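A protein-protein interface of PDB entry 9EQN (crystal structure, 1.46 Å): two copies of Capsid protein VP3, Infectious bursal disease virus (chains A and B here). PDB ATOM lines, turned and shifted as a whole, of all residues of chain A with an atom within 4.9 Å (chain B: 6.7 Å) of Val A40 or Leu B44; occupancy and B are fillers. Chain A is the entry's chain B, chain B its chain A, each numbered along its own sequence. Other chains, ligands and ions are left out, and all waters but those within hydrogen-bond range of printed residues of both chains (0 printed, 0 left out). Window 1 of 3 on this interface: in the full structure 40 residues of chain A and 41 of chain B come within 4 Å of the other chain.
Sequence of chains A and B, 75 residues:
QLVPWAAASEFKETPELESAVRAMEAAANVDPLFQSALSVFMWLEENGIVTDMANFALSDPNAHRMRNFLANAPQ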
ATOM      1  N   SER A  36      10.530  -1.300  10.605  1.00  0.00           N
ATOM      2  CA  SER A  36       9.123  -1.078  10.934  1.00  0.00           C
ATOM      3  C   SER A  36       8.940  -0.837  12.425  1.00  0.00           C
ATOM      4  O   SER A  36       8.196   0.065  12.834  1.00  0.00           O
ATOM      5  CB  SER A  36       8.285  -2.284  10.499  1.00  0.00           C
ATOM      6  OG  SER A  36       8.297  -2.440   9.085  1.00  0.00           O
ATOM      7  N   ALA A  37       9.601  -1.648  13.256  1.00  0.00           N
ATOM      8  CA  ALA A  37       9.502  -1.459  14.697  1.00  0.00           C
ATOM      9  C   ALA A  37      10.095  -0.120  15.115  1.00  0.00           C
ATOM     10  O   ALA A  37       9.519   0.587  15.954  1.00  0.00           O
ATOM     11  CB  ALA A  37      10.205  -2.609  15.415  1.00  0.00           C
ATOM     12  N   LEU A  38      11.246   0.241  14.549  1.00  0.00           N
ATOM     13  CA  LEU A  38      11.855   1.532  14.847  1.00  0.00           C
ATOM     14  C   LEU A  38      10.942   2.681  14.450  1.00  0.00           C
ATOM     15  O   LEU A  38      10.818   3.665  15.190  1.00  0.00           O
ATOM     16  CB  LEU A  38      13.208   1.649  14.138  1.00  0.00           C
ATOM     17  CG  LEU A  38      13.866   3.029  14.179  1.00  0.00           C
ATOM     18  CD1 LEU A  38      14.179   3.436  15.600  1.00  0.00           C
ATOM     19  CD2 LEU A  38      15.132   3.031  13.350  1.00  0.00           C
ATOM     20  N   SER A  39      10.289   2.572  13.286  1.00  0.00           N
ATOM     21  CA  SER A  39       9.376   3.626  12.842  1.00  0.00           C
ATOM     22  C   SER A  39       8.214   3.796  13.809  1.00  0.00           C
ATOM     23  O   SER A  39       7.795   4.926  14.091  1.00  0.00           O
ATOM     24  CB  SER A  39       8.873   3.336  11.426  1.00  0.00           C
ATOM     25  OG  SER A  39       9.929   3.463  10.490  1.00  0.00           O
ATOM     26  N   VAL A  40       7.689   2.690  14.340  1.00  0.00           N
ATOM     27  CA  VAL A  40       6.615   2.785  15.326  1.00  0.00           C
ATOM     28  C   VAL A  40       7.132   3.413  16.613  1.00  0.00           C
ATOM     29  O   VAL A  40       6.506   4.313  17.185  1.00  0.00           O
ATOM     30  CB  VAL A  40       5.994   1.401  15.586  1.00  0.00           C
ATOM     31  CG1 VAL A  40       4.982   1.485  16.721  1.00  0.00           C
ATOM     32  CG2 VAL A  40       5.352   0.867  14.331  1.00  0.00           C
ATOM     33  N   PHE A  41       8.284   2.932  17.082  1.00  0.00           N
ATOM     34  CA  PHE A  41       8.946   3.466  18.268  1.00  0.00           C
ATOM     35  C   PHE A  41       9.085   4.984  18.173  1.00  0.00           C
ATOM     36  O   PHE A  41       8.667   5.715  19.075  1.00  0.00           O
ATOM     37  CB  PHE A  41      10.311   2.785  18.361  1.00  0.00           C
ATOM     38  CG  PHE A  41      11.006   2.921  19.689  1.00  0.00           C
ATOM     39  CD1 PHE A  41      10.808   1.984  20.693  1.00  0.00           C
ATOM     40  CD2 PHE A  41      11.913   3.932  19.908  1.00  0.00           C
ATOM     41  CE1 PHE A  41      11.477   2.090  21.896  1.00  0.00           C
ATOM     42  CE2 PHE A  41      12.589   4.047  21.113  1.00  0.00           C
ATOM     43  CZ  PHE A  41      12.368   3.124  22.107  1.00  0.00           C
ATOM     44  N   MET A  42       9.642   5.475  17.062  1.00  0.00           N
ATOM     45  CA  MET A  42       9.805   6.915  16.884  1.00  0.00           C
ATOM     46  C   MET A  42       8.459   7.622  16.761  1.00  0.00           C
ATOM     47  O   MET A  42       8.297   8.745  17.250  1.00  0.00           O
ATOM     48  CB  MET A  42      10.658   7.181  15.644  1.00  0.00           C
ATOM     49  CG  MET A  42      12.113   6.773  15.795  1.00  0.00           C
ATOM     50  SD  MET A  42      12.777   7.315  17.376  1.00  0.00           S
ATOM     51  CE  MET A  42      14.328   6.437  17.421  1.00  0.00           C
ATOM     52  N   TRP A  43       7.484   6.980  16.114  1.00  0.00           N
ATOM     53  CA  TRP A  43       6.165   7.582  15.957  1.00  0.00           C
ATOM     54  C   TRP A  43       5.483   7.770  17.305  1.00  0.00           C
ATOM     55  O   TRP A  43       4.818   8.787  17.531  1.00  0.00           O
ATOM     56  CB  TRP A  43       5.343   6.690  15.018  1.00  0.00           C
ATOM     57  CG  TRP A  43       3.864   6.958  14.857  1.00  0.00           C
ATOM     58  CD1 TRP A  43       3.278   7.892  14.054  1.00  0.00           C
ATOM     59  CD2 TRP A  43       2.798   6.191  15.426  1.00  0.00           C
ATOM     60  NE1 TRP A  43       1.900   7.785  14.127  1.00  0.00           N
ATOM     61  CE2 TRP A  43       1.584   6.746  14.963  1.00  0.00           C
ATOM     62  CE3 TRP A  43       2.753   5.106  16.305  1.00  0.00           C
ATOM     63  CZ2 TRP A  43       0.346   6.244  15.338  1.00  0.00           C
ATOM     64  CZ3 TRP A  43       1.519   4.603  16.682  1.00  0.00           C
ATOM     65  CH2 TRP A  43       0.329   5.181  16.203  1.00  0.00           C
ATOM     66  N   LEU A  44       5.645   6.807  18.213  1.00  0.00           N
ATOM     67  CA  LEU A  44       5.074   6.954  19.550  1.00  0.00           C
ATOM     68  C   LEU A  44       5.645   8.176  20.258  1.00  0.00           C
ATOM     69  O   LEU A  44       4.905   8.983  20.836  1.00  0.00           O
ATOM     70  CB  LEU A  44       5.324   5.686  20.371  1.00  0.00           C
ATOM     71  CG  LEU A  44       4.620   4.399  19.943  1.00  0.00           C
ATOM     72  CD1 LEU A  44       5.115   3.242  20.780  1.00  0.00           C
ATOM     73  CD2 LEU A  44       3.117   4.560  20.104  1.00  0.00           C
ATOM     74  N   SER B  39       8.994  -1.367  26.538  1.00  0.00           N
ATOM     75  CA  SER B  39       7.919  -2.289  26.888  1.00  0.00           C
ATOM     76  C   SER B  39       6.898  -2.402  25.761  1.00  0.00           C
ATOM     77  O   SER B  39       6.459  -3.509  25.424  1.00  0.00           O
ATOM     78  CB  SER B  39       7.250  -1.855  28.191  1.00  0.00           C
ATOM     79  OG  SER B  39       8.172  -1.832  29.269  1.00  0.00           O
ATOM     80  N   VAL B  40       6.519  -1.276  25.150  1.00  0.00           N
ATOM     81  CA  VAL B  40       5.600  -1.324  24.011  1.00  0.00           C
ATOM     82  C   VAL B  40       6.241  -2.051  22.842  1.00  0.00           C
ATOM     83  O   VAL B  40       5.603  -2.883  22.184  1.00  0.00           O
ATOM     84  CB  VAL B  40       5.153   0.093  23.598  1.00  0.00           C
ATOM     85  CG1 VAL B  40       4.371   0.053  22.277  1.00  0.00           C
ATOM     86  CG2 VAL B  40       4.312   0.716  24.682  1.00  0.00           C
ATOM     87  N   PHE B  41       7.512  -1.748  22.572  1.00  0.00           N
ATOM     88  CA  PHE B  41       8.252  -2.381  21.481  1.00  0.00           C
ATOM     89  C   PHE B  41       8.199  -3.898  21.594  1.00  0.00           C
ATOM     90  O   PHE B  41       7.922  -4.601  20.613  1.00  0.00           O
ATOM     91  CB  PHE B  41       9.686  -1.858  21.544  1.00  0.00           C
ATOM     92  CG  PHE B  41      10.610  -2.390  20.489  1.00  0.00           C
ATOM     93  CD1 PHE B  41      11.333  -3.546  20.708  1.00  0.00           C
ATOM     94  CD2 PHE B  41      10.818  -1.689  19.314  1.00  0.00           C
ATOM     95  CE1 PHE B  41      12.209  -4.017  19.755  1.00  0.00           C
ATOM     96  CE2 PHE B  41      11.699  -2.152  18.362  1.00  0.00           C
ATOM     97  CZ  PHE B  41      12.389  -3.325  18.579  1.00  0.00           C
ATOM     98  N   MET B  42       8.445  -4.423  22.797  1.00  0.00           N
ATOM     99  CA  MET B  42       8.418  -5.869  22.992  1.00  0.00           C
ATOM    100  C   MET B  42       7.004  -6.412  22.855  1.00  0.00           C
ATOM    101  O   MET B  42       6.799  -7.490  22.281  1.00  0.00           O
ATOM    102  CB  MET B  42       8.999  -6.209  24.360  1.00  0.00           C
ATOM    103  CG  MET B  42      10.495  -5.904  24.482  1.00  0.00           C
ATOM    104  SD  MET B  42      11.146  -6.168  26.134  1.00  0.00           S
ATOM    105  CE  MET B  42      11.043  -7.952  26.285  1.00  0.00           C
ATOM    106  N   TRP B  43       6.016  -5.661  23.353  1.00  0.00           N
ATOM    107  CA  TRP B  43       4.618  -6.073  23.281  1.00  0.00           C
ATOM    108  C   TRP B  43       4.141  -6.168  21.836  1.00  0.00           C
ATOM    109  O   TRP B  43       3.404  -7.094  21.478  1.00  0.00           O
ATOM    110  CB  TRP B  43       3.792  -5.065  24.090  1.00  0.00           C
ATOM    111  CG  TRP B  43       2.291  -5.157  24.020  1.00  0.00           C
ATOM    112  CD1 TRP B  43       1.478  -6.025  24.691  1.00  0.00           C
ATOM    113  CD2 TRP B  43       1.428  -4.275  23.302  1.00  0.00           C
ATOM    114  NE1 TRP B  43       0.165  -5.756  24.409  1.00  0.00           N
ATOM    115  CE2 TRP B  43       0.103  -4.680  23.563  1.00  0.00           C
ATOM    116  CE3 TRP B  43       1.646  -3.172  22.469  1.00  0.00           C
ATOM    117  CZ2 TRP B  43      -0.999  -4.028  23.008  1.00  0.00           C
ATOM    118  CZ3 TRP B  43       0.555  -2.531  21.919  1.00  0.00           C
ATOM    119  CH2 TRP B  43      -0.753  -2.963  22.184  1.00  0.00           C
ATOM    120  N   LEU B  44       4.567  -5.228  20.988  1.00  0.00           N
ATOM    121  CA  LEU B  44       4.209  -5.287  19.572  1.00  0.00           C
ATOM    122  C   LEU B  44       4.793  -6.530  18.915  1.00  0.00           C
ATOM    123  O   LEU B  44       4.106  -7.220  18.151  1.00  0.00           O
ATOM    124  CB  LEU B  44       4.736  -4.048  18.847  1.00  0.00           C
ATOM    125  CG  LEU B  44       4.145  -2.682  19.177  1.00  0.00           C
ATOM    126  CD1 LEU B  44       4.969  -1.595  18.488  1.00  0.00           C
ATOM    127  CD2 LEU B  44       2.672  -2.616  18.768  1.00  0.00           C
ATOM    128  N   GLU B  45       6.062  -6.832  19.197  1.00  0.00           N
ATOM    129  CA  GLU B  45       6.694  -7.991  18.580  1.00  0.00           C
ATOM    130  C   GLU B  45       6.076  -9.290  19.087  1.00  0.00           C
ATOM    131  O   GLU B  45       5.748 -10.184  18.295  1.00  0.00           O
ATOM    132  CB  GLU B  45       8.205  -7.958  18.831  1.00  0.00           C
ATOM    133  CG  GLU B  45       9.008  -8.908  17.971  1.00  0.00           C
ATOM    134  CD  GLU B  45       8.959 -10.330  18.480  1.00  0.00           C
ATOM    135  OE1 GLU B  45       8.760 -10.505  19.701  1.00  0.00           O
ATOM    136  OE2 GLU B  45       9.113 -11.269  17.667  1.00  0.00           O
ATOM    137  N   GLU B  46       5.902  -9.411  20.409  1.00  0.00           N
ATOM    138  CA  GLU B  46       5.381 -10.650  20.978  1.00  0.00           C
ATOM    139  C   GLU B  46       3.985 -10.969  20.465  1.00  0.00           C
ATOM    140  O   GLU B  46       3.616 -12.147  20.344  1.00  0.00           O
ATOM    141  CB  GLU B  46       5.389 -10.574  22.505  1.00  0.00           C
ATOM    142  CG  GLU B  46       6.793 -10.587  23.084  1.00  0.00           C
ATOM    143  CD  GLU B  46       6.842 -10.163  24.538  1.00  0.00           C
ATOM    144  OE1 GLU B  46       5.770  -9.991  25.154  1.00  0.00           O
ATOM    145  OE2 GLU B  46       7.959  -9.996  25.063  1.00  0.00           O
ATOM    146  N   ASN B  47       3.203  -9.949  20.149  1.00  0.00           N
ATOM    147  CA  ASN B  47       1.847 -10.157  19.658  1.00  0.00           C
ATOM    148  C   ASN B  47       1.732 -10.094  18.140  1.00  0.00           C
ATOM    149  O   ASN B  47       0.622 -10.172  17.613  1.00  0.00           O
ATOM    150  CB  ASN B  47       0.884  -9.177  20.331  1.00  0.00           C
ATOM    151  CG  ASN B  47       0.695  -9.491  21.800  1.00  0.00           C
ATOM    152  OD1 ASN B  47       0.202 -10.562  22.155  1.00  0.00           O
ATOM    153  ND2 ASN B  47       1.089  -8.564  22.663  1.00  0.00           N
ATOM    154  N   GLY B  48       2.852  -9.957  17.430  1.00  0.00           N
ATOM    155  CA  GLY B  48       2.839 -10.036  15.981  1.00  0.00           C
ATOM    156  C   GLY B  48       2.210  -8.865  15.269  1.00  0.00           C
ATOM    157  O   GLY B  48       1.701  -9.038  14.156  1.00  0.00           O
ATOM    158  N   ILE B  49       2.233  -7.675  15.865  1.00  0.00           N
ATOM    159  CA  ILE B  49       1.562  -6.519  15.283  1.00  0.00           C
ATOM    160  C   ILE B  49       2.534  -5.390  14.935  1.00  0.00           C
ATOM    161  O   ILE B  49       2.129  -4.243  14.829  1.00  0.00           O
ATOM    162  CB  ILE B  49       0.389  -6.039  16.156  1.00  0.00           C
ATOM    163  CG1 ILE B  49       0.872  -5.702  17.565  1.00  0.00           C
ATOM    164  CG2 ILE B  49      -0.710  -7.095  16.177  1.00  0.00           C
ATOM    165  CD1 ILE B  49      -0.099  -4.879  18.337  1.00  0.00           C
ATOM    166  N   VAL B  50       3.815  -5.713  14.734  1.00  0.00           N
ATOM    167  CA  VAL B  50       4.797  -4.698  14.359  1.00  0.00           C
ATOM    168  C   VAL B  50       4.445  -4.074  13.014  1.00  0.00           C
ATOM    169  O   VAL B  50       4.337  -2.848  12.892  1.00  0.00           O
ATOM    170  CB  VAL B  50       6.216  -5.294  14.351  1.00  0.00           C
ATOM    171  CG1 VAL B  50       7.181  -4.332  13.682  1.00  0.00           C
ATOM    172  CG2 VAL B  50       6.654  -5.600  15.767  1.00  0.00           C
ATOM    173  N   THR B  51       4.280  -4.905  11.980  1.00  0.00           N
ATOM    174  CA  THR B  51       3.958  -4.360  10.665  1.00  0.00           C
ATOM    175  C   THR B  51       2.547  -3.778  10.627  1.00  0.00           C
ATOM    176  O   THR B  51       2.322  -2.744   9.989  1.00  0.00           O
ATOM    177  CB  THR B  51       4.175  -5.404   9.564  1.00  0.00           C
ATOM    178  OG1 THR B  51       3.293  -6.512   9.762  1.00  0.00           O
ATOM    179  CG2 THR B  51       5.608  -5.895   9.590  1.00  0.00           C
ATOM    180  N   ASP B  52       1.589  -4.411  11.313  1.00  0.00           N
ATOM    181  CA  ASP B  52       0.241  -3.845  11.389  1.00  0.00           C
ATOM    182  C   ASP B  52       0.272  -2.427  11.951  1.00  0.00           C
ATOM    183  O   ASP B  52      -0.377  -1.516  11.424  1.00  0.00           O
ATOM    184  CB  ASP B  52      -0.654  -4.722  12.264  1.00  0.00           C
ATOM    185  CG  ASP B  52      -0.605  -6.194  11.886  1.00  0.00           C
ATOM    186  OD1 ASP B  52       0.502  -6.769  11.806  1.00  0.00           O
ATOM    187  OD2 ASP B  52      -1.686  -6.779  11.681  1.00  0.00           O
ATOM    188  N   MET B  53       1.020  -2.228  13.036  1.00  0.00           N
ATOM    189  CA  MET B  53       1.084  -0.911  13.656  1.00  0.00           C
ATOM    190  C   MET B  53       1.878   0.067  12.803  1.00  0.00           C
ATOM    191  O   MET B  53       1.534   1.255  12.726  1.00  0.00           O
ATOM    192  CB  MET B  53       1.691  -1.018  15.048  1.00  0.00           C
ATOM    193  CG  MET B  53       1.698   0.281  15.822  1.00  0.00           C
ATOM    194  SD  MET B  53       0.044   0.761  16.297  1.00  0.00           S
ATOM    195  CE  MET B  53      -0.211  -0.373  17.633  1.00  0.00           C
ATOM    196  N   ALA B  54       2.950  -0.403  12.165  1.00  0.00           N
ATOM    197  CA  ALA B  54       3.709   0.473  11.281  1.00  0.00           C
ATOM    198  C   ALA B  54       2.850   0.945  10.120  1.00  0.00           C
ATOM    199  O   ALA B  54       2.877   2.128   9.755  1.00  0.00           O
ATOM    200  CB  ALA B  54       4.957  -0.245  10.767  1.00  0.00           C
ATOM    201  N   ASN B  55       2.073   0.033   9.532  1.00  0.00           N
ATOM    202  CA  ASN B  55       1.175   0.420   8.447  1.00  0.00           C
ATOM    203  C   ASN B  55       0.121   1.408   8.932  1.00  0.00           C
ATOM    204  O   ASN B  55      -0.195   2.383   8.238  1.00  0.00           O
ATOM    205  CB  ASN B  55       0.506  -0.817   7.849  1.00  0.00           C
ATOM    206  CG  ASN B  55       1.461  -1.670   7.039  1.00  0.00           C
ATOM    207  OD1 ASN B  55       2.444  -1.179   6.486  1.00  0.00           O
ATOM    208  ND2 ASN B  55       1.170  -2.964   6.963  1.00  0.00           N
ATOM    209  N   ALA B  57       0.433   3.528  11.422  1.00  0.00           N
ATOM    210  CA  ALA B  57       1.069   4.811  11.702  1.00  0.00           C
ATOM    211  C   ALA B  57       1.267   5.631  10.436  1.00  0.00           C
ATOM    212  O   ALA B  57       1.247   6.865  10.489  1.00  0.00           O
ATOM    213  CB  ALA B  57       2.396   4.600  12.436  1.00  0.00           C
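Hydrophobic or aromatic side chains of chain B that line the printed part of chain A: Val B40, Phe B41, Leu B44, Val B50, Met B53, Ala B54 and Ala B57.
Among the printed residues, 10 pairs touch across the chains.
The backbone carbonyl oxygen of Leu B44 is in hydrogen-bond range of the backbone NH of Ile B49 (3.0 Å).
Val A40 touches Leu B44, and with the chains exchanged Leu A44 touches Val B40.
Phe B41 touches its own counterpart, Phe A41.
Of the 10 pairs that touch across the chains among the printed residues, 3 have their exchanged pair printed and touching as well.
Ser A39 touches none of the printed residues of chain B.
Of chain B, only Leu B44, Met B53 and Ala B54 come within 4 Å of Val A40.
Printed residues of chain B within 4 Å of Trp A43: Ala B57.
Trp B43 touches none of the printed residues of chain A.
Printed residues of chain A within 4 Å of Val B50: Ser A36 and Ala A37.
Of the printed residues of chain A, Met B53 touches Val A40 (3.6 Å).
Of the printed residues of chain A, Ala B57 touches Trp A43.
The nearest residue of chain B that does not touch Val A40 is Val B50 (4.1 Å).
Among the printed residues, pairs that only touch across the chains: Ser A36 with Val B50 (3.9 Å), Ser A36 with Ala B54 (3.9 Å), Ala A37 with Phe B41 (3.3 Å), Ala A37 with Val B50 (3.6 Å), Val A40 with Leu B44 (3.6 Å), Val A40 with Met B53 (3.6 Å), Val A40 with Ala B54 (3.5 Å), Phe A41 with Phe B41 (3.9 Å), Trp A43 with Ala B57 (3.4 Å) and Leu A44 with Val B40 (3.6 Å).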
